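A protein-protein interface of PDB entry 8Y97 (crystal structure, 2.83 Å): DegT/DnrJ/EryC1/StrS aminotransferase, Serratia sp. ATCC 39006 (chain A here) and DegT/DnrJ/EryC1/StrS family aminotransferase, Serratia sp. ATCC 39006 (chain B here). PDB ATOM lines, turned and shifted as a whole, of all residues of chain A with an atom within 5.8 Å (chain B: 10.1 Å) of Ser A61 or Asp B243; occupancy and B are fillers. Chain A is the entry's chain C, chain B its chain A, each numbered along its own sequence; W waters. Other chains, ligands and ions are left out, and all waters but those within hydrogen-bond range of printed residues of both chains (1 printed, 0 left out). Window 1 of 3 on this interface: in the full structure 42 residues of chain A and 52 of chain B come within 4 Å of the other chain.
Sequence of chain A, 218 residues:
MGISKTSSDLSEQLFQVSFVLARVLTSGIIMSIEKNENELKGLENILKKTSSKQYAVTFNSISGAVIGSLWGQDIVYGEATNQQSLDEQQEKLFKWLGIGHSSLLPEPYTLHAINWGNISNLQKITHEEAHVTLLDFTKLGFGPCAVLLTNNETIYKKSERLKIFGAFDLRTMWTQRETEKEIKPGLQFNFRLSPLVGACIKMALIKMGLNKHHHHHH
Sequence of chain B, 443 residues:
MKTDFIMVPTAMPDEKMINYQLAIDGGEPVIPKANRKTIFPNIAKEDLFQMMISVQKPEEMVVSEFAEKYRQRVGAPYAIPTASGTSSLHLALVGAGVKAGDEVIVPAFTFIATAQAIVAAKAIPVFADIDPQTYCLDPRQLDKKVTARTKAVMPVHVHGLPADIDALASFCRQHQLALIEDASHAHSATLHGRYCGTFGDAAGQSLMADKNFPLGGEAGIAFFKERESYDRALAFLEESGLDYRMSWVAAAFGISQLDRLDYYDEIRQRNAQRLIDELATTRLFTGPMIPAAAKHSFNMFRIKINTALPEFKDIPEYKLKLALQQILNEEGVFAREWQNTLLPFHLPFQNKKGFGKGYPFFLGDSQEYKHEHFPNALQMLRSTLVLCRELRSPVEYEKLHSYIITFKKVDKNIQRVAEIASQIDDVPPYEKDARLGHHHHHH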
ATOM      1  N   PHE A  59      -2.744  27.714  20.935  1.00  0.00           N
ATOM      2  CA  PHE A  59      -2.181  27.172  19.710  1.00  0.00           C
ATOM      3  C   PHE A  59      -1.649  28.315  18.851  1.00  0.00           C
ATOM      4  O   PHE A  59      -2.064  29.460  19.015  1.00  0.00           O
ATOM      5  CB  PHE A  59      -3.239  26.366  18.949  1.00  0.00           C
ATOM      6  CG  PHE A  59      -3.777  25.161  19.706  1.00  0.00           C
ATOM      7  CD1 PHE A  59      -3.133  23.930  19.636  1.00  0.00           C
ATOM      8  CD2 PHE A  59      -4.924  25.262  20.484  1.00  0.00           C
ATOM      9  CE1 PHE A  59      -3.622  22.834  20.326  1.00  0.00           C
ATOM     10  CE2 PHE A  59      -5.408  24.164  21.176  1.00  0.00           C
ATOM     11  CZ  PHE A  59      -4.756  22.952  21.093  1.00  0.00           C
ATOM     12  N   ASN A  60      -0.739  27.980  17.926  1.00  0.00           N
ATOM     13  CA  ASN A  60      -0.186  28.942  16.984  1.00  0.00           C
ATOM     14  C   ASN A  60      -0.945  28.869  15.660  1.00  0.00           C
ATOM     15  O   ASN A  60      -0.482  29.402  14.656  1.00  0.00           O
ATOM     16  CB  ASN A  60       1.310  28.727  16.783  1.00  0.00           C
ATOM     17  CG  ASN A  60       1.638  27.456  16.032  1.00  0.00           C
ATOM     18  OD1 ASN A  60       0.794  26.909  15.310  1.00  0.00           O
ATOM     19  ND2 ASN A  60       2.869  26.981  16.166  1.00  0.00           N
ATOM     20  N   SER A  61      -2.103  28.197  15.668  1.00  0.00           N
ATOM     21  CA  SER A  61      -2.894  27.992  14.468  1.00  0.00           C
ATOM     22  C   SER A  61      -4.287  27.504  14.856  1.00  0.00           C
ATOM     23  O   SER A  61      -4.441  26.785  15.842  1.00  0.00           O
ATOM     24  CB  SER A  61      -2.223  27.017  13.534  1.00  0.00           C
ATOM     25  OG  SER A  61      -3.012  26.804  12.372  1.00  0.00           O
ATOM     26  N   ILE A  62      -5.293  27.902  14.068  1.00  0.00           N
ATOM     27  CA  ILE A  62      -6.657  27.445  14.282  1.00  0.00           C
ATOM     28  C   ILE A  62      -6.711  25.933  14.063  1.00  0.00           C
ATOM     29  O   ILE A  62      -7.475  25.240  14.730  1.00  0.00           O
ATOM     30  CB  ILE A  62      -7.666  28.206  13.395  1.00  0.00           C
ATOM     31  CG1 ILE A  62      -9.115  27.899  13.789  1.00  0.00           C
ATOM     32  CG2 ILE A  62      -7.429  27.948  11.905  1.00  0.00           C
ATOM     33  CD1 ILE A  62      -9.453  28.209  15.237  1.00  0.00           C
ATOM     34  N   SER A  63      -5.879  25.440  13.136  1.00  0.00           N
ATOM     35  CA  SER A  63      -5.785  24.020  12.845  1.00  0.00           C
ATOM     36  C   SER A  63      -5.450  23.234  14.111  1.00  0.00           C
ATOM     37  O   SER A  63      -6.018  22.172  14.350  1.00  0.00           O
ATOM     38  CB  SER A  63      -4.776  23.757  11.754  1.00  0.00           C
ATOM     39  OG  SER A  63      -5.162  24.388  10.539  1.00  0.00           O
ATOM     40  N   GLY A  64      -4.533  23.773  14.924  1.00  0.00           N
ATOM     41  CA  GLY A  64      -4.122  23.125  16.158  1.00  0.00           C
ATOM     42  C   GLY A  64      -5.263  23.025  17.168  1.00  0.00           C
ATOM     43  O   GLY A  64      -5.365  22.038  17.891  1.00  0.00           O
ATOM     44  N   ALA A  65      -6.109  24.063  17.214  1.00  0.00           N
ATOM     45  CA  ALA A  65      -7.256  24.086  18.105  1.00  0.00           C
ATOM     46  C   ALA A  65      -8.313  23.098  17.620  1.00  0.00           C
ATOM     47  O   ALA A  65      -8.952  22.429  18.427  1.00  0.00           O
ATOM     48  CB  ALA A  65      -7.810  25.491  18.194  1.00  0.00           C
ATOM     49  N   VAL A  66      -8.484  23.022  16.295  1.00  0.00           N
ATOM     50  CA  VAL A  66      -9.433  22.111  15.677  1.00  0.00           C
ATOM     51  C   VAL A  66      -9.018  20.669  15.958  1.00  0.00           C
ATOM     52  O   VAL A  66      -9.825  19.880  16.442  1.00  0.00           O
ATOM     53  CB  VAL A  66      -9.537  22.393  14.165  1.00  0.00           C
ATOM     54  CG1 VAL A  66     -10.131  21.220  13.395  1.00  0.00           C
ATOM     55  CG2 VAL A  66     -10.319  23.669  13.886  1.00  0.00           C
ATOM     56  N   GLN A  89     -12.360  25.733   4.678  1.00  0.00           N
ATOM     57  CA  GLN A  89     -11.027  25.396   5.154  1.00  0.00           C
ATOM     58  C   GLN A  89     -11.094  24.214   6.121  1.00  0.00           C
ATOM     59  O   GLN A  89     -10.337  23.254   5.975  1.00  0.00           O
ATOM     60  CB  GLN A  89     -10.327  26.579   5.823  1.00  0.00           C
ATOM     61  CG  GLN A  89      -8.811  26.421   5.861  1.00  0.00           C
ATOM     62  CD  GLN A  89      -8.112  27.435   6.740  1.00  0.00           C
ATOM     63  OE1 GLN A  89      -8.299  28.649   6.600  1.00  0.00           O
ATOM     64  NE2 GLN A  89      -7.295  26.942   7.658  1.00  0.00           N
ATOM     65  N   THR A 138      -6.602  35.071  14.919  1.00  0.00           N
ATOM     66  CA  THR A 138      -5.684  35.355  13.826  1.00  0.00           C
ATOM     67  C   THR A 138      -5.945  36.744  13.240  1.00  0.00           C
ATOM     68  O   THR A 138      -5.004  37.442  12.869  1.00  0.00           O
ATOM     69  CB  THR A 138      -5.807  34.265  12.759  1.00  0.00           C
ATOM     70  OG1 THR A 138      -5.484  33.053  13.431  1.00  0.00           O
ATOM     71  CG2 THR A 138      -4.862  34.468  11.589  1.00  0.00           C
ATOM     72  N   PRO A 144      -1.031  34.081  13.443  1.00  0.00           N
ATOM     73  CA  PRO A 144      -1.985  32.994  13.673  1.00  0.00           C
ATOM     74  C   PRO A 144      -1.989  32.518  15.124  1.00  0.00           C
ATOM     75  O   PRO A 144      -0.945  32.171  15.670  1.00  0.00           O
ATOM     76  CB  PRO A 144      -1.528  31.893  12.694  1.00  0.00           C
ATOM     77  CG  PRO A 144      -0.696  32.626  11.664  1.00  0.00           C
ATOM     78  CD  PRO A 144      -0.008  33.732  12.444  1.00  0.00           C
ATOM     79  N   CYS A 145      -3.178  32.510  15.736  1.00  0.00           N
ATOM     80  CA  CYS A 145      -3.334  32.089  17.117  1.00  0.00           C
ATOM     81  C   CYS A 145      -4.757  31.594  17.360  1.00  0.00           C
ATOM     82  O   CYS A 145      -5.711  32.136  16.808  1.00  0.00           O
ATOM     83  CB  CYS A 145      -3.023  33.226  18.080  1.00  0.00           C
ATOM     84  SG  CYS A 145      -3.383  32.819  19.808  1.00  0.00           S
ATOM     85  N   ALA A 146      -4.878  30.562  18.200  1.00  0.00           N
ATOM     86  CA  ALA A 146      -6.171  30.025  18.589  1.00  0.00           C
ATOM     87  C   ALA A 146      -6.090  29.480  20.010  1.00  0.00           C
ATOM     88  O   ALA A 146      -5.024  29.063  20.458  1.00  0.00           O
ATOM     89  CB  ALA A 146      -6.605  28.959  17.613  1.00  0.00           C
ATOM     90  N   PHE A 191       2.395  23.277  17.531  1.00  0.00           N
ATOM     91  CA  PHE A 191       1.381  24.316  17.571  1.00  0.00           C
ATOM     92  C   PHE A 191       1.630  25.231  18.769  1.00  0.00           C
ATOM     93  O   PHE A 191       0.730  25.957  19.181  1.00  0.00           O
ATOM     94  CB  PHE A 191      -0.012  23.678  17.615  1.00  0.00           C
ATOM     95  CG  PHE A 191      -0.449  22.943  16.354  1.00  0.00           C
ATOM     96  CD1 PHE A 191      -0.238  23.489  15.091  1.00  0.00           C
ATOM     97  CD2 PHE A 191      -1.084  21.707  16.438  1.00  0.00           C
ATOM     98  CE1 PHE A 191      -0.649  22.816  13.950  1.00  0.00           C
ATOM     99  CE2 PHE A 191      -1.491  21.039  15.294  1.00  0.00           C
ATOM    100  CZ  PHE A 191      -1.271  21.592  14.053  1.00  0.00           C
ATOM    101  N   GLU B  59       1.125  42.550   7.778  1.00  0.00           N
ATOM    102  CA  GLU B  59       1.778  41.403   8.396  1.00  0.00           C
ATOM    103  C   GLU B  59       2.322  40.445   7.336  1.00  0.00           C
ATOM    104  O   GLU B  59       3.413  39.904   7.501  1.00  0.00           O
ATOM    105  CB  GLU B  59       0.835  40.697   9.374  1.00  0.00           C
ATOM    106  CG  GLU B  59      -0.463  40.187   8.753  1.00  0.00           C
ATOM    107  CD  GLU B  59      -1.473  39.654   9.758  1.00  0.00           C
ATOM    108  OE1 GLU B  59      -1.105  39.436  10.933  1.00  0.00           O
ATOM    109  OE2 GLU B  59      -2.645  39.472   9.365  1.00  0.00           O
ATOM    110  N   ILE B  80       9.340  28.861   1.572  1.00  0.00           N
ATOM    111  CA  ILE B  80       8.045  29.122   2.182  1.00  0.00           C
ATOM    112  C   ILE B  80       8.261  29.375   3.671  1.00  0.00           C
ATOM    113  O   ILE B  80       8.826  28.528   4.362  1.00  0.00           O
ATOM    114  CB  ILE B  80       7.066  27.952   1.956  1.00  0.00           C
ATOM    115  CG1 ILE B  80       6.801  27.700   0.474  1.00  0.00           C
ATOM    116  CG2 ILE B  80       5.763  28.175   2.726  1.00  0.00           C
ATOM    117  CD1 ILE B  80       6.038  26.417   0.189  1.00  0.00           C
ATOM    118  N   PRO B  81       7.810  30.530   4.214  1.00  0.00           N
ATOM    119  CA  PRO B  81       7.849  30.766   5.657  1.00  0.00           C
ATOM    120  C   PRO B  81       6.725  29.988   6.338  1.00  0.00           C
ATOM    121  O   PRO B  81       5.643  29.841   5.771  1.00  0.00           O
ATOM    122  CB  PRO B  81       7.673  32.288   5.768  1.00  0.00           C
ATOM    123  CG  PRO B  81       6.842  32.654   4.555  1.00  0.00           C
ATOM    124  CD  PRO B  81       7.229  31.660   3.471  1.00  0.00           C
ATOM    125  N   THR B  82       6.991  29.489   7.551  1.00  0.00           N
ATOM    126  CA  THR B  82       6.023  28.666   8.257  1.00  0.00           C
ATOM    127  C   THR B  82       6.103  28.922   9.761  1.00  0.00           C
ATOM    128  O   THR B  82       7.015  29.591  10.241  1.00  0.00           O
ATOM    129  CB  THR B  82       6.268  27.203   7.894  1.00  0.00           C
ATOM    130  OG1 THR B  82       5.292  26.439   8.595  1.00  0.00           O
ATOM    131  CG2 THR B  82       7.647  26.717   8.289  1.00  0.00           C
ATOM    132  N   ALA B  83       5.132  28.363  10.493  1.00  0.00           N
ATOM    133  CA  ALA B  83       4.944  28.635  11.910  1.00  0.00           C
ATOM    134  C   ALA B  83       5.957  27.874  12.764  1.00  0.00           C
ATOM    135  O   ALA B  83       6.113  28.179  13.945  1.00  0.00           O
ATOM    136  CB  ALA B  83       3.532  28.270  12.314  1.00  0.00           C
ATOM    137  N   SER B  84       6.629  26.879  12.172  1.00  0.00           N
ATOM    138  CA  SER B  84       7.493  25.991  12.930  1.00  0.00           C
ATOM    139  C   SER B  84       8.430  25.230  11.999  1.00  0.00           C
ATOM    140  O   SER B  84       8.194  25.145  10.795  1.00  0.00           O
ATOM    141  CB  SER B  84       6.676  25.027  13.742  1.00  0.00           C
ATOM    142  OG  SER B  84       5.908  24.187  12.892  1.00  0.00           O
ATOM    143  N   SER B  87       6.573  22.006  10.724  1.00  0.00           N
ATOM    144  CA  SER B  87       5.716  22.264   9.579  1.00  0.00           C
ATOM    145  C   SER B  87       6.541  22.420   8.302  1.00  0.00           C
ATOM    146  O   SER B  87       6.097  22.007   7.232  1.00  0.00           O
ATOM    147  CB  SER B  87       4.845  23.468   9.828  1.00  0.00           C
ATOM    148  OG  SER B  87       5.592  24.533  10.397  1.00  0.00           O
ATOM    149  N   SER B  88       7.736  23.016   8.418  1.00  0.00           N
ATOM    150  CA  SER B  88       8.612  23.207   7.271  1.00  0.00           C
ATOM    151  C   SER B  88       9.037  21.855   6.706  1.00  0.00           C
ATOM    152  O   SER B  88       9.044  21.666   5.491  1.00  0.00           O
ATOM    153  CB  SER B  88       9.817  24.044   7.613  1.00  0.00           C
ATOM    154  OG  SER B  88      10.680  23.370   8.516  1.00  0.00           O
ATOM    155  N   HIS B  90       7.450  19.019   7.113  1.00  0.00           N
ATOM    156  CA  HIS B  90       6.245  18.426   6.552  1.00  0.00           C
ATOM    157  C   HIS B  90       6.052  18.932   5.124  1.00  0.00           C
ATOM    158  O   HIS B  90       5.844  18.138   4.209  1.00  0.00           O
ATOM    159  CB  HIS B  90       5.042  18.694   7.466  1.00  0.00           C
ATOM    160  CG  HIS B  90       3.737  18.178   6.948  1.00  0.00           C
ATOM    161  ND1 HIS B  90       2.529  18.716   7.335  1.00  0.00           N
ATOM    162  CD2 HIS B  90       3.442  17.186   6.093  1.00  0.00           C
ATOM    163  CE1 HIS B  90       1.547  18.069   6.725  1.00  0.00           C
ATOM    164  NE2 HIS B  90       2.078  17.137   5.965  1.00  0.00           N
ATOM    165  N   LEU B  91       6.139  20.255   4.945  1.00  0.00           N
ATOM    166  CA  LEU B  91       5.956  20.876   3.644  1.00  0.00           C
ATOM    167  C   LEU B  91       7.100  20.502   2.705  1.00  0.00           C
ATOM    168  O   LEU B  91       6.895  20.413   1.498  1.00  0.00           O
ATOM    169  CB  LEU B  91       5.841  22.392   3.800  1.00  0.00           C
ATOM    170  CG  LEU B  91       4.565  22.910   4.470  1.00  0.00           C
ATOM    171  CD1 LEU B  91       4.638  24.424   4.568  1.00  0.00           C
ATOM    172  CD2 LEU B  91       3.309  22.482   3.728  1.00  0.00           C
ATOM    173  N   GLU B 218       8.273  31.007  17.986  1.00  0.00           N
ATOM    174  CA  GLU B 218       8.144  29.837  17.135  1.00  0.00           C
ATOM    175  C   GLU B 218       8.116  30.285  15.678  1.00  0.00           C
ATOM    176  O   GLU B 218       7.449  31.263  15.347  1.00  0.00           O
ATOM    177  CB  GLU B 218       6.870  29.067  17.486  1.00  0.00           C
ATOM    178  CG  GLU B 218       6.809  28.614  18.942  1.00  0.00           C
ATOM    179  CD  GLU B 218       7.733  27.470  19.313  1.00  0.00           C
ATOM    180  OE1 GLU B 218       8.288  26.816  18.400  1.00  0.00           O
ATOM    181  OE2 GLU B 218       7.891  27.234  20.530  1.00  0.00           O
ATOM    182  N   PHE B 236      -0.577  21.733  -1.559  1.00  0.00           N
ATOM    183  CA  PHE B 236      -0.932  20.913  -0.411  1.00  0.00           C
ATOM    184  C   PHE B 236      -1.639  21.767   0.641  1.00  0.00           C
ATOM    185  O   PHE B 236      -2.619  21.323   1.235  1.00  0.00           O
ATOM    186  CB  PHE B 236       0.303  20.226   0.179  1.00  0.00           C
ATOM    187  CG  PHE B 236       0.050  19.524   1.507  1.00  0.00           C
ATOM    188  CD1 PHE B 236      -0.461  18.229   1.546  1.00  0.00           C
ATOM    189  CD2 PHE B 236       0.319  20.163   2.713  1.00  0.00           C
ATOM    190  CE1 PHE B 236      -0.693  17.596   2.759  1.00  0.00           C
ATOM    191  CE2 PHE B 236       0.081  19.526   3.921  1.00  0.00           C
ATOM    192  CZ  PHE B 236      -0.420  18.243   3.943  1.00  0.00           C
ATOM    193  N   LEU B 237      -1.130  22.981   0.876  1.00  0.00           N
ATOM    194  CA  LEU B 237      -1.707  23.881   1.863  1.00  0.00           C
ATOM    195  C   LEU B 237      -3.137  24.245   1.467  1.00  0.00           C
ATOM    196  O   LEU B 237      -3.996  24.393   2.331  1.00  0.00           O
ATOM    197  CB  LEU B 237      -0.838  25.129   2.028  1.00  0.00           C
ATOM    198  CG  LEU B 237       0.482  24.932   2.782  1.00  0.00           C
ATOM    199  CD1 LEU B 237       1.390  26.135   2.613  1.00  0.00           C
ATOM    200  CD2 LEU B 237       0.240  24.666   4.257  1.00  0.00           C
ATOM    201  N   GLU B 238      -3.373  24.390   0.157  1.00  0.00           N
ATOM    202  CA  GLU B 238      -4.698  24.687  -0.366  1.00  0.00           C
ATOM    203  C   GLU B 238      -5.631  23.507  -0.096  1.00  0.00           C
ATOM    204  O   GLU B 238      -6.744  23.701   0.386  1.00  0.00           O
ATOM    205  CB  GLU B 238      -4.592  25.028  -1.855  1.00  0.00           C
ATOM    206  CG  GLU B 238      -5.920  25.374  -2.527  1.00  0.00           C
ATOM    207  CD  GLU B 238      -6.572  26.679  -2.096  1.00  0.00           C
ATOM    208  OE1 GLU B 238      -5.983  27.427  -1.285  1.00  0.00           O
ATOM    209  OE2 GLU B 238      -7.686  26.952  -2.592  1.00  0.00           O
ATOM    210  N   GLU B 239      -5.160  22.289  -0.393  1.00  0.00           N
ATOM    211  CA  GLU B 239      -5.981  21.091  -0.313  1.00  0.00           C
ATOM    212  C   GLU B 239      -6.153  20.637   1.135  1.00  0.00           C
ATOM    213  O   GLU B 239      -7.259  20.283   1.540  1.00  0.00           O
ATOM    214  CB  GLU B 239      -5.364  19.962  -1.138  1.00  0.00           C
ATOM    215  CG  GLU B 239      -5.382  20.234  -2.639  1.00  0.00           C
ATOM    216  CD  GLU B 239      -4.804  19.111  -3.481  1.00  0.00           C
ATOM    217  OE1 GLU B 239      -4.422  18.065  -2.914  1.00  0.00           O
ATOM    218  OE2 GLU B 239      -4.735  19.287  -4.716  1.00  0.00           O
ATOM    219  N   SER B 240      -5.052  20.628   1.896  1.00  0.00           N
ATOM    220  CA  SER B 240      -5.038  20.103   3.254  1.00  0.00           C
ATOM    221  C   SER B 240      -5.907  20.952   4.179  1.00  0.00           C
ATOM    222  O   SER B 240      -6.538  20.420   5.089  1.00  0.00           O
ATOM    223  CB  SER B 240      -3.629  20.012   3.790  1.00  0.00           C
ATOM    224  OG  SER B 240      -3.056  21.305   3.933  1.00  0.00           O
ATOM    225  N   GLY B 241      -5.907  22.273   3.954  1.00  0.00           N
ATOM    226  CA  GLY B 241      -6.632  23.207   4.799  1.00  0.00           C
ATOM    227  C   GLY B 241      -5.853  23.544   6.069  1.00  0.00           C
ATOM    228  O   GLY B 241      -6.401  24.142   6.993  1.00  0.00           O
ATOM    229  N   LEU B 242      -4.570  23.162   6.099  1.00  0.00           N
ATOM    230  CA  LEU B 242      -3.701  23.446   7.227  1.00  0.00           C
ATOM    231  C   LEU B 242      -3.240  24.899   7.162  1.00  0.00           C
ATOM    232  O   LEU B 242      -2.884  25.392   6.095  1.00  0.00           O
ATOM    233  CB  LEU B 242      -2.510  22.489   7.209  1.00  0.00           C
ATOM    234  CG  LEU B 242      -2.783  21.066   7.699  1.00  0.00           C
ATOM    235  CD1 LEU B 242      -1.697  20.118   7.223  1.00  0.00           C
ATOM    236  CD2 LEU B 242      -2.880  21.039   9.216  1.00  0.00           C
ATOM    237  N   ASP B 243      -3.262  25.567   8.320  1.00  0.00           N
ATOM    238  CA  ASP B 243      -2.741  26.916   8.460  1.00  0.00           C
ATOM    239  C   ASP B 243      -1.373  26.834   9.133  1.00  0.00           C
ATOM    240  O   ASP B 243      -1.290  26.718  10.354  1.00  0.00           O
ATOM    241  CB  ASP B 243      -3.720  27.798   9.221  1.00  0.00           C
ATOM    242  CG  ASP B 243      -3.314  29.253   9.401  1.00  0.00           C
ATOM    243  OD1 ASP B 243      -2.294  29.663   8.808  1.00  0.00           O
ATOM    244  OD2 ASP B 243      -4.023  29.968  10.141  1.00  0.00           O
ATOM    245  N   TYR B 244      -0.311  26.891   8.316  1.00  0.00           N
ATOM    246  CA  TYR B 244       1.063  26.815   8.792  1.00  0.00           C
ATOM    247  C   TYR B 244       1.762  28.164   8.606  1.00  0.00           C
ATOM    248  O   TYR B 244       2.968  28.206   8.372  1.00  0.00           O
ATOM    249  CB  TYR B 244       1.833  25.736   8.019  1.00  0.00           C
ATOM    250  CG  TYR B 244       1.702  24.278   8.447  1.00  0.00           C
ATOM    251  CD1 TYR B 244       1.451  23.912   9.765  1.00  0.00           C
ATOM    252  CD2 TYR B 244       1.900  23.257   7.523  1.00  0.00           C
ATOM    253  CE1 TYR B 244       1.365  22.581  10.142  1.00  0.00           C
ATOM    254  CE2 TYR B 244       1.813  21.924   7.886  1.00  0.00           C
ATOM    255  CZ  TYR B 244       1.547  21.582   9.200  1.00  0.00           C
ATOM    256  OH  TYR B 244       1.468  20.266   9.556  1.00  0.00           O
ATOM    257  N   ARG B 245       1.015  29.269   8.729  1.00  0.00           N
ATOM    258  CA  ARG B 245       1.551  30.586   8.419  1.00  0.00           C
ATOM    259  C   ARG B 245       2.382  31.114   9.588  1.00  0.00           C
ATOM    260  O   ARG B 245       2.132  30.773  10.741  1.00  0.00           O
ATOM    261  CB  ARG B 245       0.432  31.570   8.066  1.00  0.00           C
ATOM    262  CG  ARG B 245      -0.197  31.325   6.701  1.00  0.00           C
ATOM    263  CD  ARG B 245      -1.342  32.290   6.440  1.00  0.00           C
ATOM    264  NE  ARG B 245      -2.418  32.105   7.423  1.00  0.00           N
ATOM    265  CZ  ARG B 245      -3.459  32.910   7.603  1.00  0.00           C
ATOM    266  NH1 ARG B 245      -3.623  33.978   6.842  1.00  0.00           N
ATOM    267  NH2 ARG B 245      -4.341  32.639   8.551  1.00  0.00           N
ATOM    268  N   MET B 246       3.364  31.965   9.260  1.00  0.00           N
ATOM    269  CA  MET B 246       4.285  32.537  10.231  1.00  0.00           C
ATOM    270  C   MET B 246       3.689  33.825  10.800  1.00  0.00           C
ATOM    271  O   MET B 246       2.881  34.484  10.148  1.00  0.00           O
ATOM    272  CB  MET B 246       5.639  32.837   9.572  1.00  0.00           C
ATOM    273  CG  MET B 246       6.705  33.377  10.513  1.00  0.00           C
ATOM    274  SD  MET B 246       8.236  33.823   9.668  1.00  0.00           S
ATOM    275  CE  MET B 246       8.860  32.197   9.229  1.00  0.00           C
ATOM    276  N   SER B 247       4.099  34.161  12.027  1.00  0.00           N
ATOM    277  CA  SER B 247       3.737  35.418  12.662  1.00  0.00           C
ATOM    278  C   SER B 247       4.697  36.515  12.207  1.00  0.00           C
ATOM    279  O   SER B 247       5.903  36.291  12.154  1.00  0.00           O
ATOM    280  CB  SER B 247       3.747  35.282  14.165  1.00  0.00           C
ATOM    281  OG  SER B 247       3.568  36.541  14.800  1.00  0.00           O
HETATM  282  O   HOH W   1      -7.620  24.771   9.331  1.00  0.00           O
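NE2 of Gln A89 lies within hydrogen-bond range of O of Gly B241 (3.0 Å).
OG of Ser A61 is in hydrogen-bond range of O of Asp B243 (2.7 Å).
N of Asp B243 lies within hydrogen-bond range of OG of Ser A63 (3.2 Å).
No residue of chain B comes within 4 Å of Ile A62.
Ser A63 touches just these residues of chain B: Gly B241, Leu B242 and Asp B243.
No residue of chain B comes within 4 Å of Gly A64.
Of the printed residues of chain B, Gln A89 touches Gly B241 and Asp B243.
Of the printed residues of chain B, Thr A138 touches Arg B245.
No residue of chain B comes within 4 Å of Ala A146.
Of the printed residues of chain A, Asp B243 touches Ser A61, Ser A63 and Gln A89.
The nearest printed residue of chain A that does not touch Asp B243 is Pro A144 (4.1 Å).
The nearest printed residue of chain A that does not touch Arg B245 is Asn A60 (4.9 Å).
Water W1 lies within hydrogen-bond range of the backbone carbonyl oxygen of Gly B241, the side-chain amide nitrogen of Gln A89 and the side-chain hydroxyl of Ser A63.
Of the 23 printed residues of chain B, 5 touch a printed residue of chain A.
Of the 14 printed residues of chain A, 5 touch a printed residue of chain B.
Among the printed residues, 9 pairs touch across the chains.
Among the printed residues, no Asp or Glu carboxylate lies within 4 Å of a Lys or Arg side-chain nitrogen of the other chain.
OG of Ser B240 lies close to N of Leu B242, 3.2 Å away.
The side-chain carboxylate of Asp B243 is in salt-bridge range of the guanidinium group of Arg B245, 2.8 Å away.
OG of Ser A61 lies close to N of Ser A63 (3.3 Å).
The side-chain hydroxyl of Thr A138 lies within hydrogen-bond range of the backbone NH of Cys A145 (3.3 Å).
Gly B241 touches Ser A63.
Leu B242 touches Ser A63.
Gln A89 touches Asp B243.
CG2 of Thr A138 touches NH2 of Arg B245 (3.6 Å).
Pro A144 touches Arg B245 (CG to O, 3.5 Å).
Pro A144 touches Met B246 (CD to O, 3.8 Å).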
